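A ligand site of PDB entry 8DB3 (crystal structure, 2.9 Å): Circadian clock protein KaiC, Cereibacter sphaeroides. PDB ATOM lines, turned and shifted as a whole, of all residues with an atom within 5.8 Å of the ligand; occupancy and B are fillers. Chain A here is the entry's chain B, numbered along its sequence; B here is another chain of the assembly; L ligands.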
ATOM      1  N   GLY A  31      -2.981  22.500  18.350  1.00  0.00           N
ATOM      2  CA  GLY A  31      -1.677  22.076  17.921  1.00  0.00           C
ATOM      3  C   GLY A  31      -1.675  20.694  17.297  1.00  0.00           C
ATOM      4  O   GLY A  31      -2.576  19.888  17.556  1.00  0.00           O
ATOM      5  N   SER A  32      -0.690  20.425  16.464  1.00  0.00           N
ATOM      6  CA  SER A  32      -0.487  19.082  15.926  1.00  0.00           C
ATOM      7  C   SER A  32       0.005  18.173  17.053  1.00  0.00           C
ATOM      8  O   SER A  32      -0.005  18.532  18.240  1.00  0.00           O
ATOM      9  CB  SER A  32       0.478  19.135  14.754  1.00  0.00           C
ATOM     10  OG  SER A  32      -0.193  19.544  13.571  1.00  0.00           O
ATOM     11  N   ALA A  33       0.434  16.971  16.696  1.00  0.00           N
ATOM     12  CA  ALA A  33       0.923  16.008  17.676  1.00  0.00           C
ATOM     13  C   ALA A  33       2.343  16.350  18.084  1.00  0.00           C
ATOM     14  O   ALA A  33       3.194  16.658  17.242  1.00  0.00           O
ATOM     15  CB  ALA A  33       0.860  14.591  17.104  1.00  0.00           C
ATOM     16  N   GLY A  34       2.602  16.289  19.388  1.00  0.00           N
ATOM     17  CA  GLY A  34       3.924  16.551  19.921  1.00  0.00           C
ATOM     18  C   GLY A  34       4.314  18.005  20.002  1.00  0.00           C
ATOM     19  O   GLY A  34       5.494  18.298  20.259  1.00  0.00           O
ATOM     20  N   CYS A  35       3.378  18.933  19.814  1.00  0.00           N
ATOM     21  CA  CYS A  35       3.690  20.349  19.856  1.00  0.00           C
ATOM     22  C   CYS A  35       3.611  20.955  21.250  1.00  0.00           C
ATOM     23  O   CYS A  35       4.020  22.107  21.436  1.00  0.00           O
ATOM     24  CB  CYS A  35       2.748  21.117  18.920  1.00  0.00           C
ATOM     25  SG  CYS A  35       2.713  20.454  17.247  1.00  0.00           S
ATOM     26  N   GLY A  36       3.081  20.220  22.218  1.00  0.00           N
ATOM     27  CA  GLY A  36       3.072  20.647  23.595  1.00  0.00           C
ATOM     28  C   GLY A  36       1.744  21.125  24.156  1.00  0.00           C
ATOM     29  O   GLY A  36       1.762  21.824  25.170  1.00  0.00           O
ATOM     30  N   LYS A  37       0.618  20.768  23.544  1.00  0.00           N
ATOM     31  CA  LYS A  37      -0.669  21.177  24.102  1.00  0.00           C
ATOM     32  C   LYS A  37      -0.886  20.553  25.476  1.00  0.00           C
ATOM     33  O   LYS A  37      -1.222  21.246  26.449  1.00  0.00           O
ATOM     34  CB  LYS A  37      -1.818  20.777  23.164  1.00  0.00           C
ATOM     35  CG  LYS A  37      -1.443  20.453  21.733  1.00  0.00           C
ATOM     36  CD  LYS A  37      -2.682  20.096  20.909  1.00  0.00           C
ATOM     37  CE  LYS A  37      -3.167  18.680  21.199  1.00  0.00           C
ATOM     38  NZ  LYS A  37      -2.449  17.677  20.360  1.00  0.00           N
ATOM     39  N   THR A  38      -0.716  19.232  25.570  1.00  0.00           N
ATOM     40  CA  THR A  38      -0.957  18.544  26.842  1.00  0.00           C
ATOM     41  C   THR A  38       0.027  19.014  27.900  1.00  0.00           C
ATOM     42  O   THR A  38      -0.332  19.165  29.069  1.00  0.00           O
ATOM     43  CB  THR A  38      -0.873  17.033  26.642  1.00  0.00           C
ATOM     44  OG1 THR A  38      -1.730  16.640  25.564  1.00  0.00           O
ATOM     45  CG2 THR A  38      -1.318  16.312  27.911  1.00  0.00           C
ATOM     46  N   LEU A  39       1.289  19.259  27.503  1.00  0.00           N
ATOM     47  CA  LEU A  39       2.265  19.741  28.472  1.00  0.00           C
ATOM     48  C   LEU A  39       1.935  21.156  28.928  1.00  0.00           C
ATOM     49  O   LEU A  39       2.109  21.480  30.107  1.00  0.00           O
ATOM     50  CB  LEU A  39       3.670  19.675  27.878  1.00  0.00           C
ATOM     51  CG  LEU A  39       4.815  19.936  28.856  1.00  0.00           C
ATOM     52  CD1 LEU A  39       4.630  19.159  30.150  1.00  0.00           C
ATOM     53  CD2 LEU A  39       6.141  19.577  28.213  1.00  0.00           C
ATOM     54  N   PHE A  40       1.463  22.010  28.018  1.00  0.00           N
ATOM     55  CA  PHE A  40       1.071  23.355  28.410  1.00  0.00           C
ATOM     56  C   PHE A  40      -0.090  23.309  29.396  1.00  0.00           C
ATOM     57  O   PHE A  40      -0.088  24.050  30.387  1.00  0.00           O
ATOM     58  CB  PHE A  40       0.702  24.169  27.169  1.00  0.00           C
ATOM     59  CG  PHE A  40       0.220  25.563  27.470  1.00  0.00           C
ATOM     60  CD1 PHE A  40      -1.114  25.817  27.727  1.00  0.00           C
ATOM     61  CD2 PHE A  40       1.111  26.628  27.469  1.00  0.00           C
ATOM     62  CE1 PHE A  40      -1.553  27.091  27.990  1.00  0.00           C
ATOM     63  CE2 PHE A  40       0.678  27.915  27.742  1.00  0.00           C
ATOM     64  CZ  PHE A  40      -0.664  28.142  27.999  1.00  0.00           C
ATOM     65  N   ASN A  71       4.098  10.520  32.116  1.00  0.00           N
ATOM     66  CA  ASN A  71       4.489  11.448  31.069  1.00  0.00           C
ATOM     67  C   ASN A  71       5.104  12.710  31.652  1.00  0.00           C
ATOM     68  O   ASN A  71       6.057  13.269  31.076  1.00  0.00           O
ATOM     69  CB  ASN A  71       3.276  11.802  30.206  1.00  0.00           C
ATOM     70  CG  ASN A  71       2.820  10.652  29.334  1.00  0.00           C
ATOM     71  OD1 ASN A  71       3.522   9.641  29.204  1.00  0.00           O
ATOM     72  ND2 ASN A  71       1.642  10.784  28.753  1.00  0.00           N
ATOM     73  N   VAL A  72       4.583  13.184  32.787  1.00  0.00           N
ATOM     74  CA  VAL A  72       5.163  14.389  33.382  1.00  0.00           C
ATOM     75  C   VAL A  72       6.132  14.121  34.527  1.00  0.00           C
ATOM     76  O   VAL A  72       6.779  15.070  35.016  1.00  0.00           O
ATOM     77  CB  VAL A  72       4.079  15.383  33.864  1.00  0.00           C
ATOM     78  CG1 VAL A  72       3.563  16.204  32.693  1.00  0.00           C
ATOM     79  CG2 VAL A  72       2.958  14.646  34.561  1.00  0.00           C
ATOM     80  N   SER A  74       9.010  12.804  34.528  1.00  0.00           N
ATOM     81  CA  SER A  74      10.396  13.045  34.157  1.00  0.00           C
ATOM     82  C   SER A  74      10.774  14.524  34.191  1.00  0.00           C
ATOM     83  O   SER A  74      11.968  14.836  34.150  1.00  0.00           O
ATOM     84  CB  SER A  74      10.654  12.472  32.760  1.00  0.00           C
ATOM     85  OG  SER A  74       9.536  12.676  31.926  1.00  0.00           O
ATOM     86  N   LEU A  75       9.800  15.426  34.265  1.00  0.00           N
ATOM     87  CA  LEU A  75      10.072  16.851  34.387  1.00  0.00           C
ATOM     88  C   LEU A  75       9.882  17.354  35.805  1.00  0.00           C
ATOM     89  O   LEU A  75       9.891  18.576  36.025  1.00  0.00           O
ATOM     90  CB  LEU A  75       9.196  17.639  33.419  1.00  0.00           C
ATOM     91  CG  LEU A  75       9.657  17.614  31.953  1.00  0.00           C
ATOM     92  CD1 LEU A  75       8.605  18.241  31.059  1.00  0.00           C
ATOM     93  CD2 LEU A  75      10.992  18.324  31.784  1.00  0.00           C
ATOM     94  N   ASP A 130      -8.602  17.024  27.997  1.00  0.00           N
ATOM     95  CA  ASP A 130      -7.695  16.353  27.075  1.00  0.00           C
ATOM     96  C   ASP A 130      -8.460  15.305  26.275  1.00  0.00           C
ATOM     97  O   ASP A 130      -9.150  14.442  26.844  1.00  0.00           O
ATOM     98  CB  ASP A 130      -6.540  15.695  27.834  1.00  0.00           C
ATOM     99  CG  ASP A 130      -5.452  15.188  26.900  1.00  0.00           C
ATOM    100  OD1 ASP A 130      -5.178  15.868  25.887  1.00  0.00           O
ATOM    101  OD2 ASP A 130      -4.877  14.119  27.179  1.00  0.00           O
ATOM    102  N   ARG A 201      10.029  25.197  17.932  1.00  0.00           N
ATOM    103  CA  ARG A 201       8.730  25.240  18.595  1.00  0.00           C
ATOM    104  C   ARG A 201       8.301  26.689  18.768  1.00  0.00           C
ATOM    105  O   ARG A 201       9.041  27.501  19.330  1.00  0.00           O
ATOM    106  CB  ARG A 201       8.814  24.543  19.965  1.00  0.00           C
ATOM    107  CG  ARG A 201       8.850  23.027  19.886  1.00  0.00           C
ATOM    108  CD  ARG A 201       8.581  22.388  21.249  1.00  0.00           C
ATOM    109  NE  ARG A 201       8.184  20.990  21.103  1.00  0.00           N
ATOM    110  CZ  ARG A 201       8.938  19.952  21.441  1.00  0.00           C
ATOM    111  NH1 ARG A 201      10.124  20.112  21.984  1.00  0.00           N
ATOM    112  NH2 ARG A 201       8.474  18.727  21.231  1.00  0.00           N
ATOM    113  N   ILE A 222      10.793  23.081  25.455  1.00  0.00           N
ATOM    114  CA  ILE A 222      10.284  22.065  26.376  1.00  0.00           C
ATOM    115  C   ILE A 222      11.492  21.296  26.900  1.00  0.00           C
ATOM    116  O   ILE A 222      11.792  20.189  26.454  1.00  0.00           O
ATOM    117  CB  ILE A 222       9.276  21.138  25.685  1.00  0.00           C
ATOM    118  CG1 ILE A 222       8.057  21.944  25.237  1.00  0.00           C
ATOM    119  CG2 ILE A 222       8.867  20.020  26.638  1.00  0.00           C
ATOM    120  CD1 ILE A 222       6.999  21.148  24.505  1.00  0.00           C
ATOM    121  N   ASP A 223      12.195  21.902  27.872  1.00  0.00           N
ATOM    122  CA  ASP A 223      13.467  21.382  28.322  1.00  0.00           C
ATOM    123  C   ASP A 223      13.321  20.761  29.713  1.00  0.00           C
ATOM    124  O   ASP A 223      12.214  20.400  30.131  1.00  0.00           O
ATOM    125  CB  ASP A 223      14.515  22.509  28.284  1.00  0.00           C
ATOM    126  CG  ASP A 223      14.027  23.777  28.976  1.00  0.00           C
ATOM    127  OD1 ASP A 223      12.797  23.956  29.084  1.00  0.00           O
ATOM    128  OD2 ASP A 223      14.876  24.586  29.393  1.00  0.00           O
ATOM    129  N   THR A 224      14.444  20.617  30.427  1.00  0.00           N
ATOM    130  CA  THR A 224      14.385  20.185  31.816  1.00  0.00           C
ATOM    131  C   THR A 224      13.623  21.170  32.683  1.00  0.00           C
ATOM    132  O   THR A 224      13.147  20.806  33.762  1.00  0.00           O
ATOM    133  CB  THR A 224      15.796  19.991  32.377  1.00  0.00           C
ATOM    134  OG1 THR A 224      16.659  19.503  31.346  1.00  0.00           O
ATOM    135  CG2 THR A 224      15.778  18.998  33.528  1.00  0.00           C
ATOM    136  N   TYR B 182      -2.210  11.035  17.013  1.00  0.00           N
ATOM    137  CA  TYR B 182      -2.660  11.633  18.256  1.00  0.00           C
ATOM    138  C   TYR B 182      -2.924  10.598  19.330  1.00  0.00           C
ATOM    139  O   TYR B 182      -2.833  10.907  20.524  1.00  0.00           O
ATOM    140  CB  TYR B 182      -3.915  12.473  18.013  1.00  0.00           C
ATOM    141  CG  TYR B 182      -3.669  13.604  17.052  1.00  0.00           C
ATOM    142  CD1 TYR B 182      -3.781  13.423  15.679  1.00  0.00           C
ATOM    143  CD2 TYR B 182      -3.314  14.859  17.512  1.00  0.00           C
ATOM    144  CE1 TYR B 182      -3.536  14.458  14.793  1.00  0.00           C
ATOM    145  CE2 TYR B 182      -3.077  15.910  16.639  1.00  0.00           C
ATOM    146  CZ  TYR B 182      -3.192  15.700  15.285  1.00  0.00           C
ATOM    147  OH  TYR B 182      -2.954  16.729  14.409  1.00  0.00           O
ATOM    148  N   ILE B 205      11.381  12.369  15.223  1.00  0.00           N
ATOM    149  CA  ILE B 205      10.562  12.115  16.410  1.00  0.00           C
ATOM    150  C   ILE B 205       9.534  13.244  16.483  1.00  0.00           C
ATOM    151  O   ILE B 205       9.834  14.338  16.951  1.00  0.00           O
ATOM    152  CB  ILE B 205      11.404  12.032  17.677  1.00  0.00           C
ATOM    153  CG1 ILE B 205      12.599  11.103  17.485  1.00  0.00           C
ATOM    154  CG2 ILE B 205      10.548  11.562  18.854  1.00  0.00           C
ATOM    155  CD1 ILE B 205      12.241   9.726  16.985  1.00  0.00           C
ATOM    156  N   VAL B 206       8.324  12.980  15.988  1.00  0.00           N
ATOM    157  CA  VAL B 206       7.290  14.010  16.012  1.00  0.00           C
ATOM    158  C   VAL B 206       6.722  14.160  17.417  1.00  0.00           C
ATOM    159  O   VAL B 206       6.475  15.282  17.885  1.00  0.00           O
ATOM    160  CB  VAL B 206       6.184  13.674  14.990  1.00  0.00           C
ATOM    161  CG1 VAL B 206       5.037  14.680  15.107  1.00  0.00           C
ATOM    162  CG2 VAL B 206       6.746  13.650  13.576  1.00  0.00           C
ATOM    163  N   LYS B 207       6.493  13.046  18.100  1.00  0.00           N
ATOM    164  CA  LYS B 207       5.972  13.045  19.462  1.00  0.00           C
ATOM    165  C   LYS B 207       6.647  11.943  20.261  1.00  0.00           C
ATOM    166  O   LYS B 207       6.977  10.881  19.731  1.00  0.00           O
ATOM    167  CB  LYS B 207       4.452  12.858  19.466  1.00  0.00           C
ATOM    168  CG  LYS B 207       3.878  12.323  20.776  1.00  0.00           C
ATOM    169  CD  LYS B 207       2.500  12.896  21.068  1.00  0.00           C
ATOM    170  CE  LYS B 207       1.412  12.160  20.295  1.00  0.00           C
ATOM    171  NZ  LYS B 207       0.062  12.372  20.901  1.00  0.00           N
ATOM    172  N   TYR B 208       6.877  12.219  21.547  1.00  0.00           N
ATOM    173  CA  TYR B 208       7.382  11.196  22.468  1.00  0.00           C
ATOM    174  C   TYR B 208       7.079  11.692  23.889  1.00  0.00           C
ATOM    175  O   TYR B 208       7.889  12.396  24.489  1.00  0.00           O
ATOM    176  CB  TYR B 208       8.861  10.946  22.253  1.00  0.00           C
ATOM    177  CG  TYR B 208       9.370   9.637  22.854  1.00  0.00           C
ATOM    178  CD1 TYR B 208       8.688   8.993  23.870  1.00  0.00           C
ATOM    179  CD2 TYR B 208      10.554   9.070  22.386  1.00  0.00           C
ATOM    180  CE1 TYR B 208       9.159   7.813  24.416  1.00  0.00           C
ATOM    181  CE2 TYR B 208      11.031   7.896  22.922  1.00  0.00           C
ATOM    182  CZ  TYR B 208      10.337   7.270  23.932  1.00  0.00           C
ATOM    183  OH  TYR B 208      10.815   6.096  24.467  1.00  0.00           O
ATOM    184  N   ARG B 209       5.918  11.307  24.397  1.00  0.00           N
ATOM    185  CA  ARG B 209       5.536  11.716  25.735  1.00  0.00           C
ATOM    186  C   ARG B 209       6.475  11.115  26.766  1.00  0.00           C
ATOM    187  O   ARG B 209       6.906   9.971  26.649  1.00  0.00           O
ATOM    188  CB  ARG B 209       4.093  11.296  26.021  1.00  0.00           C
ATOM    189  CG  ARG B 209       3.087  11.790  24.984  1.00  0.00           C
ATOM    190  CD  ARG B 209       1.830  12.371  25.641  1.00  0.00           C
ATOM    191  NE  ARG B 209       0.959  13.011  24.670  1.00  0.00           N
ATOM    192  CZ  ARG B 209      -0.364  13.090  24.778  1.00  0.00           C
ATOM    193  NH1 ARG B 209      -1.006  12.582  25.818  1.00  0.00           N
ATOM    194  NH2 ARG B 209      -1.057  13.711  23.822  1.00  0.00           N
ATOM    195  N   GLY B 210       6.812  11.913  27.786  1.00  0.00           N
ATOM    196  CA  GLY B 210       7.565  11.432  28.916  1.00  0.00           C
ATOM    197  C   GLY B 210       9.068  11.409  28.746  1.00  0.00           C
ATOM    198  O   GLY B 210       9.749  10.795  29.573  1.00  0.00           O
ATOM    199  N   THR B 211       9.601  12.042  27.708  1.00  0.00           N
ATOM    200  CA  THR B 211      11.050  12.026  27.518  1.00  0.00           C
ATOM    201  C   THR B 211      11.476  13.196  26.648  1.00  0.00           C
ATOM    202  O   THR B 211      10.732  13.652  25.790  1.00  0.00           O
ATOM    203  CB  THR B 211      11.532  10.722  26.877  1.00  0.00           C
ATOM    204  OG1 THR B 211      12.957  10.732  26.786  1.00  0.00           O
ATOM    205  CG2 THR B 211      10.959  10.576  25.476  1.00  0.00           C
ATOM    206  N   ALA B 212      12.709  13.651  26.887  1.00  0.00           N
ATOM    207  CA  ALA B 212      13.392  14.505  25.929  1.00  0.00           C
ATOM    208  C   ALA B 212      13.976  13.654  24.812  1.00  0.00           C
ATOM    209  O   ALA B 212      14.135  12.437  24.938  1.00  0.00           O
ATOM    210  CB  ALA B 212      14.496  15.311  26.622  1.00  0.00           C
ATOM    211  N   HIS B 213      14.298  14.309  23.706  1.00  0.00           N
ATOM    212  CA  HIS B 213      14.831  13.628  22.531  1.00  0.00           C
ATOM    213  C   HIS B 213      15.258  14.683  21.528  1.00  0.00           C
ATOM    214  O   HIS B 213      15.089  15.887  21.741  1.00  0.00           O
ATOM    215  CB  HIS B 213      13.787  12.686  21.928  1.00  0.00           C
ATOM    216  CG  HIS B 213      12.507  13.359  21.564  1.00  0.00           C
ATOM    217  ND1 HIS B 213      11.292  12.988  22.084  1.00  0.00           N
ATOM    218  CD2 HIS B 213      12.257  14.415  20.747  1.00  0.00           C
ATOM    219  CE1 HIS B 213      10.340  13.768  21.591  1.00  0.00           C
ATOM    220  NE2 HIS B 213      10.904  14.643  20.781  1.00  0.00           N
ATOM    221  N   THR B 215      14.596  16.711  18.346  1.00  0.00           N
ATOM    222  CA  THR B 215      13.424  17.147  17.603  1.00  0.00           C
ATOM    223  C   THR B 215      13.695  17.298  16.119  1.00  0.00           C
ATOM    224  O   THR B 215      12.743  17.273  15.326  1.00  0.00           O
ATOM    225  CB  THR B 215      12.917  18.490  18.151  1.00  0.00           C
ATOM    226  OG1 THR B 215      13.973  19.461  18.100  1.00  0.00           O
ATOM    227  CG2 THR B 215      12.438  18.337  19.575  1.00  0.00           C
HETATM  228  P1  LIG L   1       0.667  16.948  22.223  1.00  0.00           P
HETATM  229  O1  LIG L   1      -0.392  17.085  23.286  1.00  0.00           O
HETATM  230  O2  LIG L   1       1.139  18.279  21.674  1.00  0.00           O
HETATM  231  O3  LIG L   1       0.406  15.867  21.206  1.00  0.00           O
HETATM  232  P2  LIG L   1       2.307  16.829  24.504  1.00  0.00           P
HETATM  233  O4  LIG L   1       2.071  15.616  25.374  1.00  0.00           O
HETATM  234  O5  LIG L   1       1.582  18.119  24.805  1.00  0.00           O
HETATM  235  O6  LIG L   1       1.964  16.390  23.002  1.00  0.00           O
HETATM  236  O7  LIG L   1       3.884  17.098  24.424  1.00  0.00           O
HETATM  237  C1  LIG L   1       4.721  16.109  23.798  1.00  0.00           C
HETATM  238  C2  LIG L   1       6.053  16.721  23.457  1.00  0.00           C
HETATM  239  O8  LIG L   1       6.545  17.415  24.622  1.00  0.00           O
HETATM  240  C3  LIG L   1       7.117  15.710  23.009  1.00  0.00           C
HETATM  241  O9  LIG L   1       7.313  15.755  21.612  1.00  0.00           O
HETATM  242  C4  LIG L   1       8.376  16.100  23.780  1.00  0.00           C
HETATM  243  O10 LIG L   1       9.353  16.739  22.981  1.00  0.00           O
HETATM  244  C5  LIG L   1       7.911  17.080  24.873  1.00  0.00           C
HETATM  245  N1  LIG L   1       8.038  16.432  26.177  1.00  0.00           N
HETATM  246  C6  LIG L   1       7.059  15.754  26.809  1.00  0.00           C
HETATM  247  N2  LIG L   1       7.516  15.270  27.988  1.00  0.00           N
HETATM  248  C7  LIG L   1       8.796  15.635  28.109  1.00  0.00           C
HETATM  249  C8  LIG L   1       9.864  15.462  29.118  1.00  0.00           C
HETATM  250  N3  LIG L   1       9.624  14.756  30.245  1.00  0.00           N
HETATM  251  N4  LIG L   1      11.069  16.011  28.850  1.00  0.00           N
HETATM  252  C9  LIG L   1      11.315  16.709  27.721  1.00  0.00           C
HETATM  253  N5  LIG L   1      10.384  16.903  26.767  1.00  0.00           N
HETATM  254  C10 LIG L   1       9.143  16.403  26.914  1.00  0.00           C
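An oxygen (O2) of the ligand is in hydrogen-bond range of the backbone NH (N) of Cys 35 (3.0 Å). The backbone NH (N) of Gly 36 lies within hydrogen-bond range of an oxygen (O2) of the ligand (2.8 Å). N of Leu 39 lies within hydrogen-bond range of O5 of the ligand, at 2.9 Å. An oxygen (O3) of the ligand sits at hydrogen-bond distance from the backbone NH (N) of Gly 34 (2.9 Å). The backbone carbonyl oxygen (O) of Gly 34 is in hydrogen-bond range of an oxygen (O9) of the ligand (3.4 Å). NZ of Lys 207 of chain B lies within salt-bridge range of O3 of the ligand (3.5 Å). N3 of the ligand lies within hydrogen-bond range of OG of Ser 74, 2.7 Å away. The guanidinium group of Arg 209 of chain B is in salt-bridge range of an oxygen (O4) of the ligand (2.9 Å). N of Gly 210 of chain B is in hydrogen-bond range of N2 of the ligand, 3.4 Å away. The backbone NH (N) of Thr 38 sits at hydrogen-bond distance from an oxygen (O5) of the ligand (2.7 Å). NZ of Lys 37 is in salt-bridge range of O3 of the ligand (3.5 Å). The side-chain hydroxyl (OG1) of Thr 38 is in hydrogen-bond range of an oxygen (O1) of the ligand (2.7 Å). O5 of the ligand is in hydrogen-bond range of N of Lys 37. N4 of the ligand lies close to N of Ala 212 of chain B. The guanidinium group (NH2) of Arg 201 sits at hydrogen-bond distance from an oxygen (O10) of the ligand (2.8 Å). NE2 of His 213 of chain B sits at hydrogen-bond distance from O10 of the ligand (3.4 Å).
The backbone carbonyl oxygen (O) of Gly 34 sits at hydrogen-bond distance from the guanidinium group (NH2) of Arg 201 (3.2 Å). O of Tyr 182 of chain B sits at hydrogen-bond distance from NZ of Lys 207 of chain B. OG1 of Thr 38 lies within hydrogen-bond range of NH2 of Arg 209 of chain B. The side-chain amino group of Lys 37 sits at hydrogen-bond distance from the backbone carbonyl oxygen of Ser 32, at 3.3 Å. The backbone carbonyl oxygen of Ser 32 lies within hydrogen-bond range of the side-chain sulfur of Cys 35 (3.5 Å). The side-chain hydroxyl (OG) of Ser 74 lies within hydrogen-bond range of the backbone carbonyl oxygen (O) of Gly 210 of chain B (3.0 Å).
The backbone carbonyl oxygen of Thr 211 of chain B lies close to a nitrogen (N5) of the ligand. Residues that only touch the ligand: Ser 32 (3.6 Å), Ala 33 (3.6 Å), Asn 71 (3.95 Å), Leu 75 (3.3 Å), Ile 222 (3.5 Å), Val 206 of chain B (3.8 Å) and Tyr 208 of chain B (3.6 Å). 21 residues have an atom within 4 Å of the ligand: Ser 32, Ala 33, Gly 34, Cys 35, Gly 36, Lys 37, Thr 38, Leu 39, Asn 71, Ser 74, Leu 75, Arg 201, Ile 222, Val 206 of chain B, Lys 207 of chain B, Tyr 208 of chain B, Arg 209 of chain B, Gly 210 of chain B, Thr 211 of chain B, Ala 212 of chain B and His 213 of chain B. The nearest printed residue that does not touch the ligand is Asp 223 (4.5 Å).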
